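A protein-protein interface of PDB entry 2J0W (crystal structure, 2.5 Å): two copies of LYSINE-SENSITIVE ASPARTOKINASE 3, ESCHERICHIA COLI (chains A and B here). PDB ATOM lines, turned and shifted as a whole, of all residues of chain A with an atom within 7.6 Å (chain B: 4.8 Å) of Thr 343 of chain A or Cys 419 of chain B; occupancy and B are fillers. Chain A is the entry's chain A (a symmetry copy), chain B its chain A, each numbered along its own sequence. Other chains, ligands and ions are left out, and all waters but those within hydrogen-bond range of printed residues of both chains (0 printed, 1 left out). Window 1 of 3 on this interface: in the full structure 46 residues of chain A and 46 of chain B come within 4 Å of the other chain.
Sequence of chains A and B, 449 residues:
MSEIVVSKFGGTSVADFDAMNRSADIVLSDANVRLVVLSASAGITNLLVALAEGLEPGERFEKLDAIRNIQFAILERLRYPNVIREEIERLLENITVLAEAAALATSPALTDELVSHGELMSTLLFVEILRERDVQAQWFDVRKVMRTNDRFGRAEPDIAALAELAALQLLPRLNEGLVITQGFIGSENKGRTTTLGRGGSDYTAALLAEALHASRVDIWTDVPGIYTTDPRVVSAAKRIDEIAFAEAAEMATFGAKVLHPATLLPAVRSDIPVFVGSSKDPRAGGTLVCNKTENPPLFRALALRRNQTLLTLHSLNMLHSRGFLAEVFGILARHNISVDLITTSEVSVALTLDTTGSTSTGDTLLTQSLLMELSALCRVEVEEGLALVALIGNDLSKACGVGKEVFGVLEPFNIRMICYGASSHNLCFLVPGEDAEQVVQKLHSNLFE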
ATOM      1  N   LEU A 310      -6.600 -21.122   6.542  1.00  0.00           N
ATOM      2  CA  LEU A 310      -6.562 -21.246   8.003  1.00  0.00           C
ATOM      3  C   LEU A 310      -6.799 -19.891   8.663  1.00  0.00           C
ATOM      4  O   LEU A 310      -5.916 -19.030   8.683  1.00  0.00           O
ATOM      5  CB  LEU A 310      -5.224 -21.814   8.506  1.00  0.00           C
ATOM      6  CG  LEU A 310      -5.197 -21.968  10.041  1.00  0.00           C
ATOM      7  CD1 LEU A 310      -6.123 -23.108  10.462  1.00  0.00           C
ATOM      8  CD2 LEU A 310      -3.776 -22.226  10.535  1.00  0.00           C
ATOM      9  N   LEU A 311      -8.005 -19.716   9.195  1.00  0.00           N
ATOM     10  CA  LEU A 311      -8.396 -18.483   9.862  1.00  0.00           C
ATOM     11  C   LEU A 311      -8.217 -18.624  11.367  1.00  0.00           C
ATOM     12  O   LEU A 311      -9.104 -19.132  12.058  1.00  0.00           O
ATOM     13  CB  LEU A 311      -9.852 -18.180   9.553  1.00  0.00           C
ATOM     14  CG  LEU A 311     -10.376 -16.883  10.150  1.00  0.00           C
ATOM     15  CD1 LEU A 311      -9.619 -15.693   9.567  1.00  0.00           C
ATOM     16  CD2 LEU A 311     -11.855 -16.788   9.853  1.00  0.00           C
ATOM     17  N   THR A 312      -7.067 -18.178  11.864  1.00  0.00           N
ATOM     18  CA  THR A 312      -6.738 -18.251  13.288  1.00  0.00           C
ATOM     19  C   THR A 312      -7.214 -17.000  14.040  1.00  0.00           C
ATOM     20  O   THR A 312      -6.892 -15.871  13.665  1.00  0.00           O
ATOM     21  CB  THR A 312      -5.212 -18.409  13.480  1.00  0.00           C
ATOM     22  OG1 THR A 312      -4.770 -19.616  12.848  1.00  0.00           O
ATOM     23  CG2 THR A 312      -4.860 -18.457  14.950  1.00  0.00           C
ATOM     24  N   LEU A 313      -7.990 -17.205  15.098  1.00  0.00           N
ATOM     25  CA  LEU A 313      -8.490 -16.084  15.883  1.00  0.00           C
ATOM     26  C   LEU A 313      -7.961 -16.034  17.310  1.00  0.00           C
ATOM     27  O   LEU A 313      -8.143 -16.960  18.103  1.00  0.00           O
ATOM     28  CB  LEU A 313     -10.014 -16.094  15.916  1.00  0.00           C
ATOM     29  CG  LEU A 313     -10.682 -15.782  14.582  1.00  0.00           C
ATOM     30  CD1 LEU A 313     -12.197 -15.739  14.757  1.00  0.00           C
ATOM     31  CD2 LEU A 313     -10.156 -14.446  14.062  1.00  0.00           C
ATOM     32  N   VAL A 339     -17.679 -24.423   9.188  1.00  0.00           N
ATOM     33  CA  VAL A 339     -16.328 -24.966   9.364  1.00  0.00           C
ATOM     34  C   VAL A 339     -16.374 -26.430   9.790  1.00  0.00           C
ATOM     35  O   VAL A 339     -17.010 -26.775  10.794  1.00  0.00           O
ATOM     36  CB  VAL A 339     -15.548 -24.184  10.441  1.00  0.00           C
ATOM     37  CG1 VAL A 339     -14.158 -24.779  10.615  1.00  0.00           C
ATOM     38  CG2 VAL A 339     -15.463 -22.725  10.046  1.00  0.00           C
ATOM     39  N   LEU A 341     -13.510 -28.197  10.365  1.00  0.00           N
ATOM     40  CA  LEU A 341     -12.410 -28.434  11.283  1.00  0.00           C
ATOM     41  C   LEU A 341     -11.939 -27.230  12.106  1.00  0.00           C
ATOM     42  O   LEU A 341     -11.474 -26.231  11.554  1.00  0.00           O
ATOM     43  CB  LEU A 341     -11.220 -29.023  10.503  1.00  0.00           C
ATOM     44  CG  LEU A 341     -11.417 -30.401   9.854  1.00  0.00           C
ATOM     45  CD1 LEU A 341     -10.230 -30.747   8.971  1.00  0.00           C
ATOM     46  CD2 LEU A 341     -11.588 -31.452  10.930  1.00  0.00           C
ATOM     47  N   ILE A 342     -12.054 -27.346  13.432  1.00  0.00           N
ATOM     48  CA  ILE A 342     -11.623 -26.300  14.357  1.00  0.00           C
ATOM     49  C   ILE A 342     -10.663 -26.868  15.398  1.00  0.00           C
ATOM     50  O   ILE A 342     -10.787 -28.030  15.811  1.00  0.00           O
ATOM     51  CB  ILE A 342     -12.809 -25.669  15.125  1.00  0.00           C
ATOM     52  CG1 ILE A 342     -13.773 -25.002  14.153  1.00  0.00           C
ATOM     53  CG2 ILE A 342     -12.294 -24.645  16.118  1.00  0.00           C
ATOM     54  CD1 ILE A 342     -14.841 -24.184  14.835  1.00  0.00           C
ATOM     55  N   THR A 343      -9.710 -26.035  15.814  1.00  0.00           N
ATOM     56  CA  THR A 343      -8.715 -26.398  16.816  1.00  0.00           C
ATOM     57  C   THR A 343      -8.496 -25.171  17.711  1.00  0.00           C
ATOM     58  O   THR A 343      -8.352 -24.060  17.199  1.00  0.00           O
ATOM     59  CB  THR A 343      -7.378 -26.835  16.141  1.00  0.00           C
ATOM     60  OG1 THR A 343      -7.082 -28.185  16.519  1.00  0.00           O
ATOM     61  CG2 THR A 343      -6.221 -25.937  16.557  1.00  0.00           C
ATOM     62  N   THR A 344      -8.485 -25.362  19.033  1.00  0.00           N
ATOM     63  CA  THR A 344      -8.292 -24.234  19.957  1.00  0.00           C
ATOM     64  C   THR A 344      -7.156 -24.399  20.958  1.00  0.00           C
ATOM     65  O   THR A 344      -6.573 -25.468  21.106  1.00  0.00           O
ATOM     66  CB  THR A 344      -9.569 -23.939  20.783  1.00  0.00           C
ATOM     67  OG1 THR A 344      -9.872 -25.059  21.624  1.00  0.00           O
ATOM     68  CG2 THR A 344     -10.748 -23.677  19.876  1.00  0.00           C
ATOM     69  N   SER A 345      -6.844 -23.304  21.633  1.00  0.00           N
ATOM     70  CA  SER A 345      -5.820 -23.285  22.666  1.00  0.00           C
ATOM     71  C   SER A 345      -6.119 -22.043  23.494  1.00  0.00           C
ATOM     72  O   SER A 345      -5.642 -20.935  23.203  1.00  0.00           O
ATOM     73  CB  SER A 345      -4.415 -23.213  22.068  1.00  0.00           C
ATOM     74  OG  SER A 345      -3.439 -23.194  23.105  1.00  0.00           O
ATOM     75  N   GLU A 346      -6.932 -22.249  24.528  1.00  0.00           N
ATOM     76  CA  GLU A 346      -7.371 -21.176  25.411  1.00  0.00           C
ATOM     77  C   GLU A 346      -8.270 -20.275  24.605  1.00  0.00           C
ATOM     78  O   GLU A 346      -9.331 -20.702  24.168  1.00  0.00           O
ATOM     79  CB  GLU A 346      -6.198 -20.368  25.944  1.00  0.00           C
ATOM     80  CG  GLU A 346      -5.306 -21.154  26.874  1.00  0.00           C
ATOM     81  CD  GLU A 346      -4.265 -20.290  27.540  1.00  0.00           C
ATOM     82  OE1 GLU A 346      -4.642 -19.455  28.395  1.00  0.00           O
ATOM     83  OE2 GLU A 346      -3.072 -20.449  27.197  1.00  0.00           O
ATOM     84  N   SER A 348      -7.421 -18.876  21.695  1.00  0.00           N
ATOM     85  CA  SER A 348      -6.926 -18.814  20.323  1.00  0.00           C
ATOM     86  C   SER A 348      -7.646 -19.927  19.583  1.00  0.00           C
ATOM     87  O   SER A 348      -7.521 -21.094  19.946  1.00  0.00           O
ATOM     88  CB  SER A 348      -5.423 -19.064  20.308  1.00  0.00           C
ATOM     89  OG  SER A 348      -4.813 -18.412  21.414  1.00  0.00           O
ATOM     90  N   VAL A 349      -8.420 -19.579  18.566  1.00  0.00           N
ATOM     91  CA  VAL A 349      -9.152 -20.593  17.817  1.00  0.00           C
ATOM     92  C   VAL A 349      -8.795 -20.592  16.327  1.00  0.00           C
ATOM     93  O   VAL A 349      -9.043 -19.616  15.625  1.00  0.00           O
ATOM     94  CB  VAL A 349     -10.663 -20.396  18.010  1.00  0.00           C
ATOM     95  CG1 VAL A 349     -10.995 -18.916  17.948  1.00  0.00           C
ATOM     96  CG2 VAL A 349     -11.433 -21.174  16.959  1.00  0.00           C
ATOM     97  N   ALA A 350      -8.199 -21.691  15.858  1.00  0.00           N
ATOM     98  CA  ALA A 350      -7.787 -21.824  14.455  1.00  0.00           C
ATOM     99  C   ALA A 350      -8.862 -22.508  13.631  1.00  0.00           C
ATOM    100  O   ALA A 350      -9.187 -23.681  13.850  1.00  0.00           O
ATOM    101  CB  ALA A 350      -6.464 -22.601  14.350  1.00  0.00           C
ATOM    102  N   LEU A 351      -9.404 -21.761  12.674  1.00  0.00           N
ATOM    103  CA  LEU A 351     -10.467 -22.254  11.807  1.00  0.00           C
ATOM    104  C   LEU A 351      -9.963 -22.748  10.443  1.00  0.00           C
ATOM    105  O   LEU A 351      -9.215 -22.040   9.761  1.00  0.00           O
ATOM    106  CB  LEU A 351     -11.494 -21.137  11.616  1.00  0.00           C
ATOM    107  CG  LEU A 351     -12.174 -20.632  12.890  1.00  0.00           C
ATOM    108  CD1 LEU A 351     -12.827 -19.297  12.625  1.00  0.00           C
ATOM    109  CD2 LEU A 351     -13.205 -21.641  13.350  1.00  0.00           C
ATOM    110  N   THR A 352     -10.381 -23.957  10.058  1.00  0.00           N
ATOM    111  CA  THR A 352      -9.988 -24.562   8.781  1.00  0.00           C
ATOM    112  C   THR A 352     -11.069 -24.315   7.734  1.00  0.00           C
ATOM    113  O   THR A 352     -12.113 -24.964   7.752  1.00  0.00           O
ATOM    114  CB  THR A 352      -9.776 -26.095   8.917  1.00  0.00           C
ATOM    115  OG1 THR A 352      -8.709 -26.363   9.837  1.00  0.00           O
ATOM    116  CG2 THR A 352      -9.428 -26.702   7.570  1.00  0.00           C
ATOM    117  N   ARG A 416       0.857 -28.031   9.927  1.00  0.00           N
ATOM    118  CA  ARG A 416       0.353 -26.755  10.423  1.00  0.00           C
ATOM    119  C   ARG A 416      -0.830 -26.827  11.373  1.00  0.00           C
ATOM    120  O   ARG A 416      -1.060 -25.913  12.180  1.00  0.00           O
ATOM    121  CB  ARG A 416      -0.037 -25.876   9.238  1.00  0.00           C
ATOM    122  CG  ARG A 416      -0.620 -24.528   9.634  1.00  0.00           C
ATOM    123  CD  ARG A 416       0.437 -23.609  10.223  1.00  0.00           C
ATOM    124  NE  ARG A 416      -0.132 -22.314  10.590  1.00  0.00           N
ATOM    125  CZ  ARG A 416      -0.756 -22.062  11.738  1.00  0.00           C
ATOM    126  NH1 ARG A 416      -0.887 -23.018  12.649  1.00  0.00           N
ATOM    127  NH2 ARG A 416      -1.268 -20.861  11.966  1.00  0.00           N
ATOM    128  N   MET A 417      -1.590 -27.903  11.274  1.00  0.00           N
ATOM    129  CA  MET A 417      -2.767 -28.032  12.105  1.00  0.00           C
ATOM    130  C   MET A 417      -3.107 -29.500  12.200  1.00  0.00           C
ATOM    131  O   MET A 417      -2.980 -30.234  11.225  1.00  0.00           O
ATOM    132  CB  MET A 417      -3.927 -27.264  11.460  1.00  0.00           C
ATOM    133  CG  MET A 417      -5.185 -27.116  12.292  1.00  0.00           C
ATOM    134  SD  MET A 417      -6.200 -28.601  12.313  1.00  0.00           S
ATOM    135  CE  MET A 417      -6.512 -28.818  10.602  1.00  0.00           C
ATOM    136  N   ILE A 418      -3.491 -29.942  13.385  1.00  0.00           N
ATOM    137  CA  ILE A 418      -3.885 -31.319  13.534  1.00  0.00           C
ATOM    138  C   ILE A 418      -5.179 -31.268  14.299  1.00  0.00           C
ATOM    139  O   ILE A 418      -5.260 -30.686  15.371  1.00  0.00           O
ATOM    140  CB  ILE A 418      -2.845 -32.143  14.297  1.00  0.00           C
ATOM    141  CG1 ILE A 418      -1.481 -31.980  13.632  1.00  0.00           C
ATOM    142  CG2 ILE A 418      -3.238 -33.615  14.263  1.00  0.00           C
ATOM    143  CD1 ILE A 418      -0.403 -32.808  14.251  1.00  0.00           C
ATOM    144  N   CYS A 419      -6.215 -31.839  13.721  1.00  0.00           N
ATOM    145  CA  CYS A 419      -7.500 -31.833  14.375  1.00  0.00           C
ATOM    146  C   CYS A 419      -7.920 -33.275  14.440  1.00  0.00           C
ATOM    147  O   CYS A 419      -8.145 -33.912  13.404  1.00  0.00           O
ATOM    148  CB  CYS A 419      -8.500 -31.014  13.566  1.00  0.00           C
ATOM    149  SG  CYS A 419     -10.081 -30.865  14.371  1.00  0.00           S
ATOM    150  N   TYR A 420      -8.006 -33.790  15.665  1.00  0.00           N
ATOM    151  CA  TYR A 420      -8.362 -35.184  15.887  1.00  0.00           C
ATOM    152  C   TYR A 420      -8.940 -35.452  17.261  1.00  0.00           C
ATOM    153  O   TYR A 420      -8.489 -34.885  18.261  1.00  0.00           O
ATOM    154  CB  TYR A 420      -7.121 -36.044  15.683  1.00  0.00           C
ATOM    155  CG  TYR A 420      -7.235 -37.473  16.148  1.00  0.00           C
ATOM    156  CD1 TYR A 420      -8.258 -38.305  15.685  1.00  0.00           C
ATOM    157  CD2 TYR A 420      -6.298 -38.005  17.030  1.00  0.00           C
ATOM    158  CE1 TYR A 420      -8.339 -39.628  16.088  1.00  0.00           C
ATOM    159  CE2 TYR A 420      -6.371 -39.326  17.439  1.00  0.00           C
ATOM    160  CZ  TYR A 420      -7.389 -40.133  16.963  1.00  0.00           C
ATOM    161  OH  TYR A 420      -7.436 -41.446  17.351  1.00  0.00           O
ATOM    162  N   GLY A 421      -9.942 -36.330  17.295  1.00  0.00           N
ATOM    163  CA  GLY A 421     -10.578 -36.710  18.547  1.00  0.00           C
ATOM    164  C   GLY A 421     -12.079 -36.544  18.572  1.00  0.00           C
ATOM    165  O   GLY A 421     -12.757 -37.112  19.419  1.00  0.00           O
ATOM    166  N   LEU B 341      -8.896 -26.552  25.665  1.00  0.00           N
ATOM    167  CA  LEU B 341      -8.681 -27.334  24.460  1.00  0.00           C
ATOM    168  C   LEU B 341      -9.931 -27.935  23.807  1.00  0.00           C
ATOM    169  O   LEU B 341     -10.623 -28.757  24.409  1.00  0.00           O
ATOM    170  CB  LEU B 341      -7.666 -28.453  24.759  1.00  0.00           C
ATOM    171  CG  LEU B 341      -6.240 -28.025  25.140  1.00  0.00           C
ATOM    172  CD1 LEU B 341      -5.427 -29.229  25.586  1.00  0.00           C
ATOM    173  CD2 LEU B 341      -5.575 -27.359  23.955  1.00  0.00           C
ATOM    174  N   ILE B 342     -10.198 -27.524  22.565  1.00  0.00           N
ATOM    175  CA  ILE B 342     -11.334 -28.023  21.794  1.00  0.00           C
ATOM    176  C   ILE B 342     -10.871 -28.558  20.441  1.00  0.00           C
ATOM    177  O   ILE B 342      -9.914 -28.040  19.848  1.00  0.00           O
ATOM    178  CB  ILE B 342     -12.384 -26.922  21.514  1.00  0.00           C
ATOM    179  CG1 ILE B 342     -12.961 -26.397  22.822  1.00  0.00           C
ATOM    180  CG2 ILE B 342     -13.501 -27.480  20.653  1.00  0.00           C
ATOM    181  CD1 ILE B 342     -14.139 -25.474  22.630  1.00  0.00           C
ATOM    182  N   THR B 343     -11.560 -29.594  19.968  1.00  0.00           N
ATOM    183  CA  THR B 343     -11.271 -30.225  18.686  1.00  0.00           C
ATOM    184  C   THR B 343     -12.615 -30.581  18.037  1.00  0.00           C
ATOM    185  O   THR B 343     -13.493 -31.124  18.709  1.00  0.00           O
ATOM    186  CB  THR B 343     -10.395 -31.503  18.878  1.00  0.00           C
ATOM    187  OG1 THR B 343      -9.163 -31.336  18.166  1.00  0.00           O
ATOM    188  CG2 THR B 343     -11.102 -32.749  18.364  1.00  0.00           C
ATOM    189  N   MET B 417      -6.862 -37.653  21.710  1.00  0.00           N
ATOM    190  CA  MET B 417      -7.212 -36.341  21.213  1.00  0.00           C
ATOM    191  C   MET B 417      -5.931 -35.602  20.912  1.00  0.00           C
ATOM    192  O   MET B 417      -4.954 -35.722  21.647  1.00  0.00           O
ATOM    193  CB  MET B 417      -8.012 -35.591  22.286  1.00  0.00           C
ATOM    194  CG  MET B 417      -8.641 -34.278  21.865  1.00  0.00           C
ATOM    195  SD  MET B 417      -7.468 -32.916  21.810  1.00  0.00           S
ATOM    196  CE  MET B 417      -6.877 -32.914  23.460  1.00  0.00           C
ATOM    197  N   ILE B 418      -5.911 -34.878  19.806  1.00  0.00           N
ATOM    198  CA  ILE B 418      -4.740 -34.102  19.488  1.00  0.00           C
ATOM    199  C   ILE B 418      -5.269 -32.742  19.120  1.00  0.00           C
ATOM    200  O   ILE B 418      -6.116 -32.604  18.252  1.00  0.00           O
ATOM    201  CB  ILE B 418      -3.946 -34.699  18.324  1.00  0.00           C
ATOM    202  CG1 ILE B 418      -3.630 -36.163  18.623  1.00  0.00           C
ATOM    203  CG2 ILE B 418      -2.637 -33.937  18.158  1.00  0.00           C
ATOM    204  CD1 ILE B 418      -2.785 -36.824  17.584  1.00  0.00           C
ATOM    205  N   CYS B 419      -4.800 -31.732  19.822  1.00  0.00           N
ATOM    206  CA  CYS B 419      -5.254 -30.391  19.549  1.00  0.00           C
ATOM    207  C   CYS B 419      -4.005 -29.591  19.302  1.00  0.00           C
ATOM    208  O   CYS B 419      -3.180 -29.418  20.207  1.00  0.00           O
ATOM    209  CB  CYS B 419      -6.023 -29.840  20.744  1.00  0.00           C
ATOM    210  SG  CYS B 419      -6.715 -28.229  20.435  1.00  0.00           S
ATOM    211  N   TYR B 420      -3.864 -29.118  18.066  1.00  0.00           N
ATOM    212  CA  TYR B 420      -2.689 -28.359  17.665  1.00  0.00           C
ATOM    213  C   TYR B 420      -2.925 -27.461  16.468  1.00  0.00           C
ATOM    214  O   TYR B 420      -3.626 -27.834  15.522  1.00  0.00           O
ATOM    215  CB  TYR B 420      -1.561 -29.334  17.352  1.00  0.00           C
ATOM    216  CG  TYR B 420      -0.364 -28.742  16.650  1.00  0.00           C
ATOM    217  CD1 TYR B 420       0.322 -27.650  17.186  1.00  0.00           C
ATOM    218  CD2 TYR B 420       0.103 -29.298  15.461  1.00  0.00           C
ATOM    219  CE1 TYR B 420       1.441 -27.131  16.557  1.00  0.00           C
ATOM    220  CE2 TYR B 420       1.221 -28.786  14.824  1.00  0.00           C
ATOM    221  CZ  TYR B 420       1.887 -27.707  15.377  1.00  0.00           C
ATOM    222  OH  TYR B 420       3.009 -27.227  14.754  1.00  0.00           O
ATOM    223  N   GLY B 421      -2.323 -26.273  16.522  1.00  0.00           N
ATOM    224  CA  GLY B 421      -2.433 -25.315  15.433  1.00  0.00           C
ATOM    225  C   GLY B 421      -2.918 -23.944  15.841  1.00  0.00           C
ATOM    226  O   GLY B 421      -2.753 -22.978  15.106  1.00  0.00           O
ATOM    227  N   ALA B 422      -3.512 -23.863  17.021  1.00  0.00           N
ATOM    228  CA  ALA B 422      -4.031 -22.604  17.514  1.00  0.00           C
ATOM    229  C   ALA B 422      -2.955 -21.729  18.142  1.00  0.00           C
ATOM    230  O   ALA B 422      -3.128 -20.519  18.257  1.00  0.00           O
ATOM    231  CB  ALA B 422      -5.144 -22.864  18.509  1.00  0.00           C
ATOM    232  N   ASN B 426       2.423 -24.367  21.629  1.00  0.00           N
ATOM    233  CA  ASN B 426       2.141 -25.699  22.162  1.00  0.00           C
ATOM    234  C   ASN B 426       1.424 -26.702  21.268  1.00  0.00           C
ATOM    235  O   ASN B 426       0.761 -26.348  20.291  1.00  0.00           O
ATOM    236  CB  ASN B 426       1.306 -25.574  23.428  1.00  0.00           C
ATOM    237  CG  ASN B 426      -0.172 -25.452  23.121  1.00  0.00           C
ATOM    238  OD1 ASN B 426      -0.780 -26.379  22.568  1.00  0.00           O
ATOM    239  ND2 ASN B 426      -0.758 -24.306  23.459  1.00  0.00           N
ATOM    240  N   LEU B 427       1.535 -27.961  21.677  1.00  0.00           N
ATOM    241  CA  LEU B 427       0.895 -29.078  21.011  1.00  0.00           C
ATOM    242  C   LEU B 427       0.460 -30.017  22.128  1.00  0.00           C
ATOM    243  O   LEU B 427       1.303 -30.604  22.812  1.00  0.00           O
ATOM    244  CB  LEU B 427       1.878 -29.796  20.094  1.00  0.00           C
ATOM    245  CG  LEU B 427       1.276 -30.946  19.281  1.00  0.00           C
ATOM    246  CD1 LEU B 427       2.150 -31.192  18.073  1.00  0.00           C
ATOM    247  CD2 LEU B 427       1.136 -32.211  20.125  1.00  0.00           C
ATOM    248  N   CYS B 428      -0.843 -30.168  22.324  1.00  0.00           N
ATOM    249  CA  CYS B 428      -1.315 -31.039  23.393  1.00  0.00           C
ATOM    250  C   CYS B 428      -2.047 -32.255  22.888  1.00  0.00           C
ATOM    251  O   CYS B 428      -2.452 -32.324  21.731  1.00  0.00           O
ATOM    252  CB  CYS B 428      -2.250 -30.275  24.320  1.00  0.00           C
ATOM    253  SG  CYS B 428      -1.682 -28.625  24.663  1.00  0.00           S
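Thr 343 of chain A touches just these residues of chain B: Ile 342 (3.7 Å), Cys 419 (3.9 Å), Tyr 420 (3.4 Å), Gly 421 (3.9 Å) and Ala 422 (3.4 Å). Cys 419 of chain B touches just these residues of chain A: Thr 343 and Thr 344. Printed residues of chain A within 4 Å of Tyr 420 of chain B: Thr 343 (3.4 Å), Met 417 (3.5 Å) and Ile 418 (3.0 Å). Of the printed residues of chain B, Ser 348 of chain A touches Ala 422. Printed residues of chain B within 4 Å of Ala 350 of chain A: Gly 421 (3.8 Å) and Ala 422 (3.99 Å). Printed residues of chain A within 4 Å of Ile 342 of chain B: Thr 343 and Thr 344. Printed residues of chain A within 4 Å of Ala 422 of chain B: Thr 343 (3.4 Å), Thr 344 (3.5 Å), Ser 345 (3.6 Å), Ser 348 (3.3 Å) and Ala 350 (3.99 Å). Glu 346 of chain A touches none of the printed residues of chain B.
Hydrophobic or aromatic side chains of chain B that line the printed part of chain A: Leu 341, Ile 342, Met 417, Ile 418, Tyr 420 and Ala 422. Printed residues of chain A that touch a printed residue of chain B: Ile 342, Thr 343, Thr 344, Ser 345, Ser 348, Ala 350, Arg 416, Met 417, Ile 418, Cys 419, Tyr 420 and Gly 421. Among the printed residues, 24 pairs touch across the chains. Among the printed residues, no Asp or Glu carboxylate lies within 4 Å of a Lys or Arg side-chain nitrogen of the other chain.
ND2 of Asn 426 of chain B sits at hydrogen-bond distance from OG of Ser 345 of chain A (2.9 Å). The backbone NH of Ile 418 of chain B sits at hydrogen-bond distance from the backbone carbonyl oxygen of Tyr 420 of chain A, 3.0 Å away. OG1 of Thr 344 of chain A lies within hydrogen-bond range of N of Ile 342 of chain B (2.7 Å). SG of Cys 419 of chain B lies within hydrogen-bond range of O of Thr 344 of chain A, at 2.8 Å. The guanidinium group of Arg 416 of chain A sits at hydrogen-bond distance from the backbone carbonyl oxygen of Gly 421 of chain B (3.1 Å). The backbone carbonyl oxygen (O) of Tyr 420 of chain B lies within hydrogen-bond range of the backbone NH (N) of Ile 418 of chain A (3.0 Å).
The side-chain hydroxyl (OG1) of Thr 343 of chain B is in hydrogen-bond range of the backbone carbonyl oxygen (O) of Ile 418 of chain B, 3.3 Å away. The side-chain hydroxyl of Ser 348 of chain A lies within hydrogen-bond range of the backbone carbonyl oxygen of Ser 345 of chain A. The side-chain sulfur (SD) of Met 417 of chain A is in hydrogen-bond range of the backbone NH (N) of Cys 419 of chain A (3.5 Å). O of Ile 342 of chain A sits at hydrogen-bond distance from SG of Cys 419 of chain A, at 3.3 Å. The backbone carbonyl oxygen (O) of Ile 342 of chain B sits at hydrogen-bond distance from the side-chain sulfur (SG) of Cys 419 of chain B (3.3 Å). The backbone carbonyl oxygen (O) of Ile 418 of chain A is in hydrogen-bond range of the side-chain hydroxyl (OG1) of Thr 343 of chain A (3.3 Å).
Ile 342 of chain A touches Thr 343 of chain B, and with the chains exchanged Thr 343 of chain A touches Ile 342 of chain B. Thr 343 of chain A touches Tyr 420 of chain B, and with the chains exchanged Tyr 420 of chain A touches Thr 343 of chain B. Thr 343 of chain A touches Gly 421 of chain B, and with the chains exchanged Gly 421 of chain A touches Thr 343 of chain B. Met 417 of chain A touches Tyr 420 of chain B, and with the chains exchanged Tyr 420 of chain A touches Met 417 of chain B. Of the 24 pairs that touch across the chains among the printed residues, 13 have their exchanged pair printed and touching as well.
Thr 343 of chain A touches Cys 419 of chain B (OG1 to SG, 3.9 Å). Thr 343 of chain A touches Tyr 420 of chain B. N of Gly 421 of chain B touches CG2 of Thr 343 of chain A, 3.9 Å away. Thr 344 of chain A touches Leu 341 of chain B. Thr 344 of chain A touches Ala 422 of chain B. CB of Ala 422 of chain B touches N of Ser 345 of chain A, at 3.6 Å. O of Ser 348 of chain A touches CB of Ala 422 of chain B (3.3 Å). CB of Ala 350 of chain A touches O of Gly 421 of chain B, 3.8 Å away. Cys 419 of chain A touches Thr 343 of chain B (SG to OG1, 3.9 Å). CG2 of Thr 343 of chain B touches N of Gly 421 of chain A, at 3.9 Å.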
